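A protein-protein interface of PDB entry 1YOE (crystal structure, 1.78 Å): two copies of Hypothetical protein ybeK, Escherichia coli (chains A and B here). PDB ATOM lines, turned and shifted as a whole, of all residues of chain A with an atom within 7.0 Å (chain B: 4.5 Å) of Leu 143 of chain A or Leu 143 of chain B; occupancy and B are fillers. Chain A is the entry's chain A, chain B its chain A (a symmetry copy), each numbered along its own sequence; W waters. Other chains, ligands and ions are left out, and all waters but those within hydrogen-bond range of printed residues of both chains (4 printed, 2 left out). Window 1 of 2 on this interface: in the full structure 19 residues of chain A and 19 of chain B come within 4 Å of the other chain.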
ATOM      1  N   GLY A  77      15.746  34.637   8.995  1.00  0.00           N
ATOM      2  CA  GLY A  77      16.009  33.220   9.207  1.00  0.00           C
ATOM      3  C   GLY A  77      17.442  32.839   9.546  1.00  0.00           C
ATOM      4  O   GLY A  77      18.224  33.638  10.075  1.00  0.00           O
ATOM      5  N   ALA A  78      17.779  31.591   9.236  1.00  0.00           N
ATOM      6  CA  ALA A  78      19.095  31.027   9.540  1.00  0.00           C
ATOM      7  C   ALA A  78      20.201  31.867   8.907  1.00  0.00           C
ATOM      8  O   ALA A  78      20.040  32.411   7.802  1.00  0.00           O
ATOM      9  CB  ALA A  78      19.168  29.596   9.044  1.00  0.00           C
ATOM     10  N   LYS A  80      23.263  30.874   8.151  1.00  0.00           N
ATOM     11  CA  LYS A  80      24.127  30.067   7.287  1.00  0.00           C
ATOM     12  C   LYS A  80      23.466  28.718   6.977  1.00  0.00           C
ATOM     13  O   LYS A  80      22.490  28.341   7.645  1.00  0.00           O
ATOM     14  CB  LYS A  80      25.494  29.855   7.968  1.00  0.00           C
ATOM     15  CG  LYS A  80      25.417  29.028   9.236  1.00  0.00           C
ATOM     16  CD  LYS A  80      26.795  28.841   9.885  1.00  0.00           C
ATOM     17  CE  LYS A  80      27.625  27.772   9.188  1.00  0.00           C
ATOM     18  NZ  LYS A  80      26.979  26.415   9.217  1.00  0.00           N
ATOM     19  N   LEU A  82      22.878  24.603   6.840  1.00  0.00           N
ATOM     20  CA  LEU A  82      22.877  23.635   7.936  1.00  0.00           C
ATOM     21  C   LEU A  82      24.261  23.122   8.326  1.00  0.00           C
ATOM     22  O   LEU A  82      24.609  23.095   9.511  1.00  0.00           O
ATOM     23  CB  LEU A  82      21.984  22.440   7.579  1.00  0.00           C
ATOM     24  CG  LEU A  82      20.520  22.780   7.290  1.00  0.00           C
ATOM     25  CD1 LEU A  82      19.767  21.492   6.981  1.00  0.00           C
ATOM     26  CD2 LEU A  82      19.865  23.525   8.471  1.00  0.00           C
ATOM     27  N   VAL A 116      11.765  30.395  11.396  1.00  0.00           N
ATOM     28  CA  VAL A 116      11.115  29.112  11.715  1.00  0.00           C
ATOM     29  C   VAL A 116       9.983  29.332  12.720  1.00  0.00           C
ATOM     30  O   VAL A 116       8.892  28.775  12.577  1.00  0.00           O
ATOM     31  CB  VAL A 116      12.136  28.049  12.183  1.00  0.00           C
ATOM     32  CG1 VAL A 116      11.426  26.795  12.713  1.00  0.00           C
ATOM     33  CG2 VAL A 116      13.035  27.669  11.017  1.00  0.00           C
ATOM     34  N   GLN A 138      17.145  26.246   0.910  1.00  0.00           N
ATOM     35  CA  GLN A 138      16.028  25.620   1.639  1.00  0.00           C
ATOM     36  C   GLN A 138      16.241  25.536   3.149  1.00  0.00           C
ATOM     37  O   GLN A 138      15.488  24.863   3.839  1.00  0.00           O
ATOM     38  CB  GLN A 138      15.736  24.224   1.043  1.00  0.00           C
ATOM     39  CG  GLN A 138      15.157  24.291  -0.391  1.00  0.00           C
ATOM     40  CD  GLN A 138      13.867  25.099  -0.474  1.00  0.00           C
ATOM     41  OE1 GLN A 138      13.006  25.010   0.417  1.00  0.00           O
ATOM     42  NE2 GLN A 138      13.725  25.889  -1.540  1.00  0.00           N
ATOM     43  N   THR A 139      17.237  26.260   3.658  1.00  0.00           N
ATOM     44  CA  THR A 139      17.666  26.151   5.061  1.00  0.00           C
ATOM     45  C   THR A 139      16.526  26.304   6.078  1.00  0.00           C
ATOM     46  O   THR A 139      16.356  25.449   6.958  1.00  0.00           O
ATOM     47  CB  THR A 139      18.749  27.191   5.337  1.00  0.00           C
ATOM     48  OG1 THR A 139      19.728  27.133   4.289  1.00  0.00           O
ATOM     49  CG2 THR A 139      19.509  26.819   6.626  1.00  0.00           C
ATOM     50  N   ASN A 140      15.753  27.380   5.959  1.00  0.00           N
ATOM     51  CA  ASN A 140      14.648  27.610   6.903  1.00  0.00           C
ATOM     52  C   ASN A 140      13.563  26.553   6.814  1.00  0.00           C
ATOM     53  O   ASN A 140      13.032  26.104   7.832  1.00  0.00           O
ATOM     54  CB  ASN A 140      14.005  28.973   6.692  1.00  0.00           C
ATOM     55  CG  ASN A 140      14.938  30.112   7.006  1.00  0.00           C
ATOM     56  OD1 ASN A 140      15.744  30.037   7.943  1.00  0.00           O
ATOM     57  ND2 ASN A 140      14.832  31.188   6.225  1.00  0.00           N
ATOM     58  N   VAL A 141      13.223  26.184   5.581  1.00  0.00           N
ATOM     59  CA  VAL A 141      12.194  25.180   5.327  1.00  0.00           C
ATOM     60  C   VAL A 141      12.599  23.838   5.940  1.00  0.00           C
ATOM     61  O   VAL A 141      11.795  23.194   6.615  1.00  0.00           O
ATOM     62  CB  VAL A 141      11.867  25.046   3.819  1.00  0.00           C
ATOM     63  CG1 VAL A 141      10.742  24.019   3.612  1.00  0.00           C
ATOM     64  CG2 VAL A 141      11.457  26.410   3.244  1.00  0.00           C
ATOM     65  N   ALA A 142      13.849  23.432   5.735  1.00  0.00           N
ATOM     66  CA  ALA A 142      14.326  22.181   6.322  1.00  0.00           C
ATOM     67  C   ALA A 142      14.264  22.211   7.849  1.00  0.00           C
ATOM     68  O   ALA A 142      13.860  21.228   8.477  1.00  0.00           O
ATOM     69  CB  ALA A 142      15.728  21.881   5.846  1.00  0.00           C
ATOM     70  N   LEU A 143      14.665  23.329   8.447  1.00  0.00           N
ATOM     71  CA  LEU A 143      14.622  23.465   9.898  1.00  0.00           C
ATOM     72  C   LEU A 143      13.187  23.362  10.406  1.00  0.00           C
ATOM     73  O   LEU A 143      12.930  22.701  11.409  1.00  0.00           O
ATOM     74  CB  LEU A 143      15.249  24.789  10.341  1.00  0.00           C
ATOM     75  CG  LEU A 143      16.775  24.797  10.184  1.00  0.00           C
ATOM     76  CD1 LEU A 143      17.278  26.223  10.389  1.00  0.00           C
ATOM     77  CD2 LEU A 143      17.445  23.817  11.158  1.00  0.00           C
ATOM     78  N   LEU A 144      12.257  23.986   9.688  1.00  0.00           N
ATOM     79  CA  LEU A 144      10.837  23.856  10.027  1.00  0.00           C
ATOM     80  C   LEU A 144      10.364  22.401   9.969  1.00  0.00           C
ATOM     81  O   LEU A 144       9.700  21.919  10.895  1.00  0.00           O
ATOM     82  CB  LEU A 144       9.993  24.711   9.077  1.00  0.00           C
ATOM     83  CG  LEU A 144       8.473  24.605   9.221  1.00  0.00           C
ATOM     84  CD1 LEU A 144       7.982  25.171  10.557  1.00  0.00           C
ATOM     85  CD2 LEU A 144       7.853  25.326   8.044  1.00  0.00           C
ATOM     86  N   LEU A 145      10.684  21.707   8.876  1.00  0.00           N
ATOM     87  CA  LEU A 145      10.245  20.316   8.692  1.00  0.00           C
ATOM     88  C   LEU A 145      10.761  19.378   9.773  1.00  0.00           C
ATOM     89  O   LEU A 145       9.992  18.601  10.346  1.00  0.00           O
ATOM     90  CB  LEU A 145      10.631  19.785   7.308  1.00  0.00           C
ATOM     91  CG  LEU A 145       9.991  20.531   6.146  1.00  0.00           C
ATOM     92  CD1 LEU A 145      10.578  20.049   4.827  1.00  0.00           C
ATOM     93  CD2 LEU A 145       8.484  20.393   6.159  1.00  0.00           C
ATOM     94  N   ASN A 146      12.050  19.479  10.066  1.00  0.00           N
ATOM     95  CA  ASN A 146      12.675  18.615  11.063  1.00  0.00           C
ATOM     96  C   ASN A 146      12.273  18.958  12.490  1.00  0.00           C
ATOM     97  O   ASN A 146      12.160  18.057  13.328  1.00  0.00           O
ATOM     98  CB  ASN A 146      14.194  18.700  10.959  1.00  0.00           C
ATOM     99  CG  ASN A 146      14.778  17.889   9.798  1.00  0.00           C
ATOM    100  OD1 ASN A 146      15.901  18.144   9.393  1.00  0.00           O
ATOM    101  ND2 ASN A 146      14.035  16.911   9.283  1.00  0.00           N
ATOM    102  N   SER A 147      12.100  20.249  12.781  1.00  0.00           N
ATOM    103  CA  SER A 147      11.790  20.663  14.155  1.00  0.00           C
ATOM    104  C   SER A 147      10.299  20.607  14.471  1.00  0.00           C
ATOM    105  O   SER A 147       9.933  20.625  15.645  1.00  0.00           O
ATOM    106  CB  SER A 147      12.317  22.052  14.525  1.00  0.00           C
ATOM    107  OG  SER A 147      11.767  23.059  13.721  1.00  0.00           O
ATOM    108  N   HIS A 148       9.456  20.527  13.443  1.00  0.00           N
ATOM    109  CA  HIS A 148       7.999  20.521  13.660  1.00  0.00           C
ATOM    110  C   HIS A 148       7.270  19.392  12.928  1.00  0.00           C
ATOM    111  O   HIS A 148       6.402  19.642  12.087  1.00  0.00           O
ATOM    112  CB  HIS A 148       7.414  21.902  13.310  1.00  0.00           C
ATOM    113  CG  HIS A 148       7.731  22.950  14.330  1.00  0.00           C
ATOM    114  ND1 HIS A 148       7.169  22.949  15.589  1.00  0.00           N
ATOM    115  CD2 HIS A 148       8.560  24.019  14.289  1.00  0.00           C
ATOM    116  CE1 HIS A 148       7.624  23.987  16.272  1.00  0.00           C
ATOM    117  NE2 HIS A 148       8.477  24.648  15.507  1.00  0.00           N
ATOM    118  N   ALA A 184      19.793  20.793   3.248  1.00  0.00           N
ATOM    119  CA  ALA A 184      18.435  21.336   3.452  1.00  0.00           C
ATOM    120  C   ALA A 184      17.488  20.975   2.315  1.00  0.00           C
ATOM    121  O   ALA A 184      16.316  20.625   2.544  1.00  0.00           O
ATOM    122  CB  ALA A 184      18.460  22.827   3.641  1.00  0.00           C
ATOM    123  N   ILE A 187      16.516  17.369   2.626  1.00  0.00           N
ATOM    124  CA  ILE A 187      15.499  17.223   3.680  1.00  0.00           C
ATOM    125  C   ILE A 187      14.095  17.548   3.140  1.00  0.00           C
ATOM    126  O   ILE A 187      13.130  16.815   3.399  1.00  0.00           O
ATOM    127  CB  ILE A 187      15.858  18.077   4.912  1.00  0.00           C
ATOM    128  CG1 ILE A 187      17.055  17.450   5.654  1.00  0.00           C
ATOM    129  CG2 ILE A 187      14.633  18.266   5.860  1.00  0.00           C
ATOM    130  CD1 ILE A 187      17.831  18.416   6.584  1.00  0.00           C
ATOM    131  N   VAL A 188      13.987  18.637   2.380  1.00  0.00           N
ATOM    132  CA  VAL A 188      12.723  19.000   1.742  1.00  0.00           C
ATOM    133  C   VAL A 188      12.210  17.884   0.825  1.00  0.00           C
ATOM    134  O   VAL A 188      11.056  17.447   0.952  1.00  0.00           O
ATOM    135  CB  VAL A 188      12.841  20.348   0.968  1.00  0.00           C
ATOM    136  CG1 VAL A 188      11.617  20.609   0.086  1.00  0.00           C
ATOM    137  CG2 VAL A 188      13.067  21.516   1.956  1.00  0.00           C
ATOM    138  N   ALA B  78      12.562  15.683  18.236  1.00  0.00           N
ATOM    139  CA  ALA B  78      12.458  15.234  16.846  1.00  0.00           C
ATOM    140  C   ALA B  78      12.130  13.745  16.782  1.00  0.00           C
ATOM    141  O   ALA B  78      12.591  12.951  17.619  1.00  0.00           O
ATOM    142  CB  ALA B  78      13.755  15.522  16.115  1.00  0.00           C
ATOM    143  N   LEU B  82      17.931  13.935  11.257  1.00  0.00           N
ATOM    144  CA  LEU B  82      17.792  15.019  10.286  1.00  0.00           C
ATOM    145  C   LEU B  82      17.579  14.554   8.848  1.00  0.00           C
ATOM    146  O   LEU B  82      16.678  15.044   8.158  1.00  0.00           O
ATOM    147  CB  LEU B  82      19.024  15.931  10.340  1.00  0.00           C
ATOM    148  CG  LEU B  82      19.296  16.585  11.696  1.00  0.00           C
ATOM    149  CD1 LEU B  82      20.528  17.474  11.576  1.00  0.00           C
ATOM    150  CD2 LEU B  82      18.083  17.400  12.188  1.00  0.00           C
ATOM    151  N   VAL B 116      13.012  21.521  21.058  1.00  0.00           N
ATOM    152  CA  VAL B 116      13.771  22.714  20.642  1.00  0.00           C
ATOM    153  C   VAL B 116      13.129  23.974  21.225  1.00  0.00           C
ATOM    154  O   VAL B 116      13.821  24.864  21.726  1.00  0.00           O
ATOM    155  CB  VAL B 116      13.942  22.782  19.106  1.00  0.00           C
ATOM    156  CG1 VAL B 116      14.541  24.129  18.676  1.00  0.00           C
ATOM    157  CG2 VAL B 116      14.852  21.652  18.652  1.00  0.00           C
ATOM    158  N   THR B 139      20.230  15.066  17.432  1.00  0.00           N
ATOM    159  CA  THR B 139      19.212  15.667  16.557  1.00  0.00           C
ATOM    160  C   THR B 139      18.608  16.970  17.101  1.00  0.00           C
ATOM    161  O   THR B 139      18.582  17.988  16.397  1.00  0.00           O
ATOM    162  CB  THR B 139      18.103  14.649  16.303  1.00  0.00           C
ATOM    163  OG1 THR B 139      18.698  13.393  15.942  1.00  0.00           O
ATOM    164  CG2 THR B 139      17.276  15.077  15.075  1.00  0.00           C
ATOM    165  N   ASN B 140      18.128  16.939  18.342  1.00  0.00           N
ATOM    166  CA  ASN B 140      17.518  18.140  18.933  1.00  0.00           C
ATOM    167  C   ASN B 140      18.505  19.279  19.111  1.00  0.00           C
ATOM    168  O   ASN B 140      18.181  20.442  18.859  1.00  0.00           O
ATOM    169  CB  ASN B 140      16.888  17.840  20.285  1.00  0.00           C
ATOM    170  CG  ASN B 140      15.715  16.901  20.185  1.00  0.00           C
ATOM    171  OD1 ASN B 140      14.933  16.956  19.227  1.00  0.00           O
ATOM    172  ND2 ASN B 140      15.577  16.028  21.185  1.00  0.00           N
ATOM    173  N   VAL B 141      19.703  18.932  19.576  1.00  0.00           N
ATOM    174  CA  VAL B 141      20.761  19.911  19.803  1.00  0.00           C
ATOM    175  C   VAL B 141      21.137  20.601  18.490  1.00  0.00           C
ATOM    176  O   VAL B 141      21.245  21.827  18.440  1.00  0.00           O
ATOM    177  CB  VAL B 141      21.997  19.287  20.497  1.00  0.00           C
ATOM    178  CG1 VAL B 141      23.056  20.370  20.763  1.00  0.00           C
ATOM    179  CG2 VAL B 141      21.580  18.613  21.813  1.00  0.00           C
ATOM    180  N   ALA B 142      21.306  19.824  17.425  1.00  0.00           N
ATOM    181  CA  ALA B 142      21.626  20.410  16.125  1.00  0.00           C
ATOM    182  C   ALA B 142      20.523  21.351  15.640  1.00  0.00           C
ATOM    183  O   ALA B 142      20.811  22.432  15.117  1.00  0.00           O
ATOM    184  CB  ALA B 142      21.888  19.320  15.110  1.00  0.00           C
ATOM    185  N   LEU B 143      19.268  20.946  15.807  1.00  0.00           N
ATOM    186  CA  LEU B 143      18.145  21.783  15.400  1.00  0.00           C
ATOM    187  C   LEU B 143      18.137  23.091  16.185  1.00  0.00           C
ATOM    188  O   LEU B 143      17.910  24.155  15.615  1.00  0.00           O
ATOM    189  CB  LEU B 143      16.819  21.043  15.584  1.00  0.00           C
ATOM    190  CG  LEU B 143      16.622  19.927  14.551  1.00  0.00           C
ATOM    191  CD1 LEU B 143      15.421  19.082  14.970  1.00  0.00           C
ATOM    192  CD2 LEU B 143      16.443  20.495  13.136  1.00  0.00           C
ATOM    193  N   LEU B 144      18.420  23.006  17.482  1.00  0.00           N
ATOM    194  CA  LEU B 144      18.547  24.215  18.301  1.00  0.00           C
ATOM    195  C   LEU B 144      19.655  25.141  17.790  1.00  0.00           C
ATOM    196  O   LEU B 144      19.445  26.352  17.647  1.00  0.00           O
ATOM    197  CB  LEU B 144      18.825  23.832  19.758  1.00  0.00           C
ATOM    198  CG  LEU B 144      19.096  24.981  20.732  1.00  0.00           C
ATOM    199  CD1 LEU B 144      17.858  25.858  20.945  1.00  0.00           C
ATOM    200  CD2 LEU B 144      19.582  24.372  22.029  1.00  0.00           C
ATOM    201  N   LEU B 145      20.839  24.581  17.538  1.00  0.00           N
ATOM    202  CA  LEU B 145      21.988  25.379  17.086  1.00  0.00           C
ATOM    203  C   LEU B 145      21.736  26.096  15.768  1.00  0.00           C
ATOM    204  O   LEU B 145      21.997  27.296  15.649  1.00  0.00           O
ATOM    205  CB  LEU B 145      23.258  24.528  16.987  1.00  0.00           C
ATOM    206  CG  LEU B 145      23.719  23.930  18.308  1.00  0.00           C
ATOM    207  CD1 LEU B 145      24.870  22.963  18.071  1.00  0.00           C
ATOM    208  CD2 LEU B 145      24.103  25.006  19.301  1.00  0.00           C
ATOM    209  N   ASN B 146      21.201  25.366  14.799  1.00  0.00           N
ATOM    210  CA  ASN B 146      20.939  25.927  13.478  1.00  0.00           C
ATOM    211  C   ASN B 146      19.767  26.897  13.459  1.00  0.00           C
ATOM    212  O   ASN B 146      19.791  27.873  12.702  1.00  0.00           O
ATOM    213  CB  ASN B 146      20.653  24.812  12.476  1.00  0.00           C
ATOM    214  CG  ASN B 146      21.911  24.087  11.988  1.00  0.00           C
ATOM    215  OD1 ASN B 146      21.807  22.981  11.480  1.00  0.00           O
ATOM    216  ND2 ASN B 146      23.082  24.708  12.120  1.00  0.00           N
ATOM    217  N   SER B 147      18.730  26.616  14.251  1.00  0.00           N
ATOM    218  CA  SER B 147      17.531  27.461  14.230  1.00  0.00           C
ATOM    219  C   SER B 147      17.639  28.672  15.152  1.00  0.00           C
ATOM    220  O   SER B 147      16.859  29.610  15.005  1.00  0.00           O
ATOM    221  CB  SER B 147      16.232  26.716  14.551  1.00  0.00           C
ATOM    222  OG  SER B 147      16.246  26.158  15.835  1.00  0.00           O
HETATM  223  O   HOH W   1      21.973  26.937   9.961  1.00  0.00           O
HETATM  224  O   HOH W   2      17.047  31.005  12.477  1.00  0.00           O
HETATM  225  O   HOH W   3      10.776  18.369  17.250  1.00  0.00           O
HETATM  226  O   HOH W   4      24.692  26.581  11.249  1.00  0.00           O
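Leu 143 of chain A touches Leu 143 of chain B (CD2 to CD2, 3.99 Å). CB of Asn 146 of chain B touches CD2 of Leu 143 of chain A (3.6 Å). Asn 146 of chain A touches Leu 143 of chain B (CB to CD2, 3.6 Å). Leu 82 of chain B touches Ile 187 of chain A (O to CG1, 3.5 Å).
Printed residues of chain B within 4 Å of Leu 82 of chain A: Asn 146 (3.4 Å). Of the printed residues of chain B, Asn 146 of chain A touches Leu 82 (3.4 Å) and Leu 143 (3.6 Å). Of the printed residues of chain B, Ile 187 of chain A touches Leu 82. Val 116 of chain B touches none of the printed residues of chain A. Thr 139 of chain B touches none of the printed residues of chain A. Printed residues of chain A within 4 Å of Leu 143 of chain B: Leu 143 and Asn 146. Printed residues of chain A within 4 Å of Asn 146 of chain B: Leu 82 and Leu 143. The nearest printed residue of chain A that does not touch Leu 143 of chain B is Ser 147 of chain A (4.04 Å). The nearest printed residue of chain B that does not touch Leu 82 of chain A is Leu 82 of chain B (6.2 Å).
O of Leu 143 of chain A is in hydrogen-bond range of OG of Ser 147 of chain A, at 2.6 Å. The backbone carbonyl oxygen of Leu 143 of chain B is in hydrogen-bond range of the side-chain hydroxyl of Ser 147 of chain B (2.6 Å).
Water W4 bridges the side-chain amide nitrogen of Asn 146 of chain B (2.6 Å) and the side-chain amino group of Lys 80 of chain A (3.1 Å). Water W1 bridges O of Lys 80 of chain A (2.8 Å) and ND2 of Asn 146 of chain B (3.3 Å). Water W2 lies within hydrogen-bond range of the backbone carbonyl oxygen of Ser 147 of chain B (2.9 Å) and the backbone NH of Ala 78 of chain A (3.4 Å). Water W3 bridges the backbone carbonyl oxygen (O) of Ser 147 of chain A and the backbone NH (N) of Ala 78 of chain B.
The side-chain amide oxygen of Asn 146 of chain B sits close to the backbone carbonyl oxygen of Leu 82 of chain A (3.4 Å). The side-chain amide oxygen (OD1) of Asn 146 of chain A lies close to the backbone carbonyl oxygen (O) of Leu 82 of chain B (3.4 Å).
Of the 19 printed residues of chain A, 4 touch a printed residue of chain B. Hydrophobic or aromatic side chains of chain A within 4 Å of the printed part of chain B: Leu 82, Leu 143 and Ile 187. Hydrophobic or aromatic side chains of chain B that line the printed part of chain A: Leu 82 and Leu 143. Among the printed residues, no Asp or Glu carboxylate lies within 4 Å of a Lys or Arg side-chain nitrogen of the other chain.
Leu 82 of chain A touches Asn 146 of chain B, and with the chains exchanged Asn 146 of chain A touches Leu 82 of chain B. Leu 143 of chain B touches its own counterpart, Leu 143 of chain A. Leu 143 of chain A touches Asn 146 of chain B, and with the chains exchanged Asn 146 of chain A touches Leu 143 of chain B. Of the 6 pairs that touch across the chains among the printed residues, 5 have their exchanged pair printed and touching as well.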
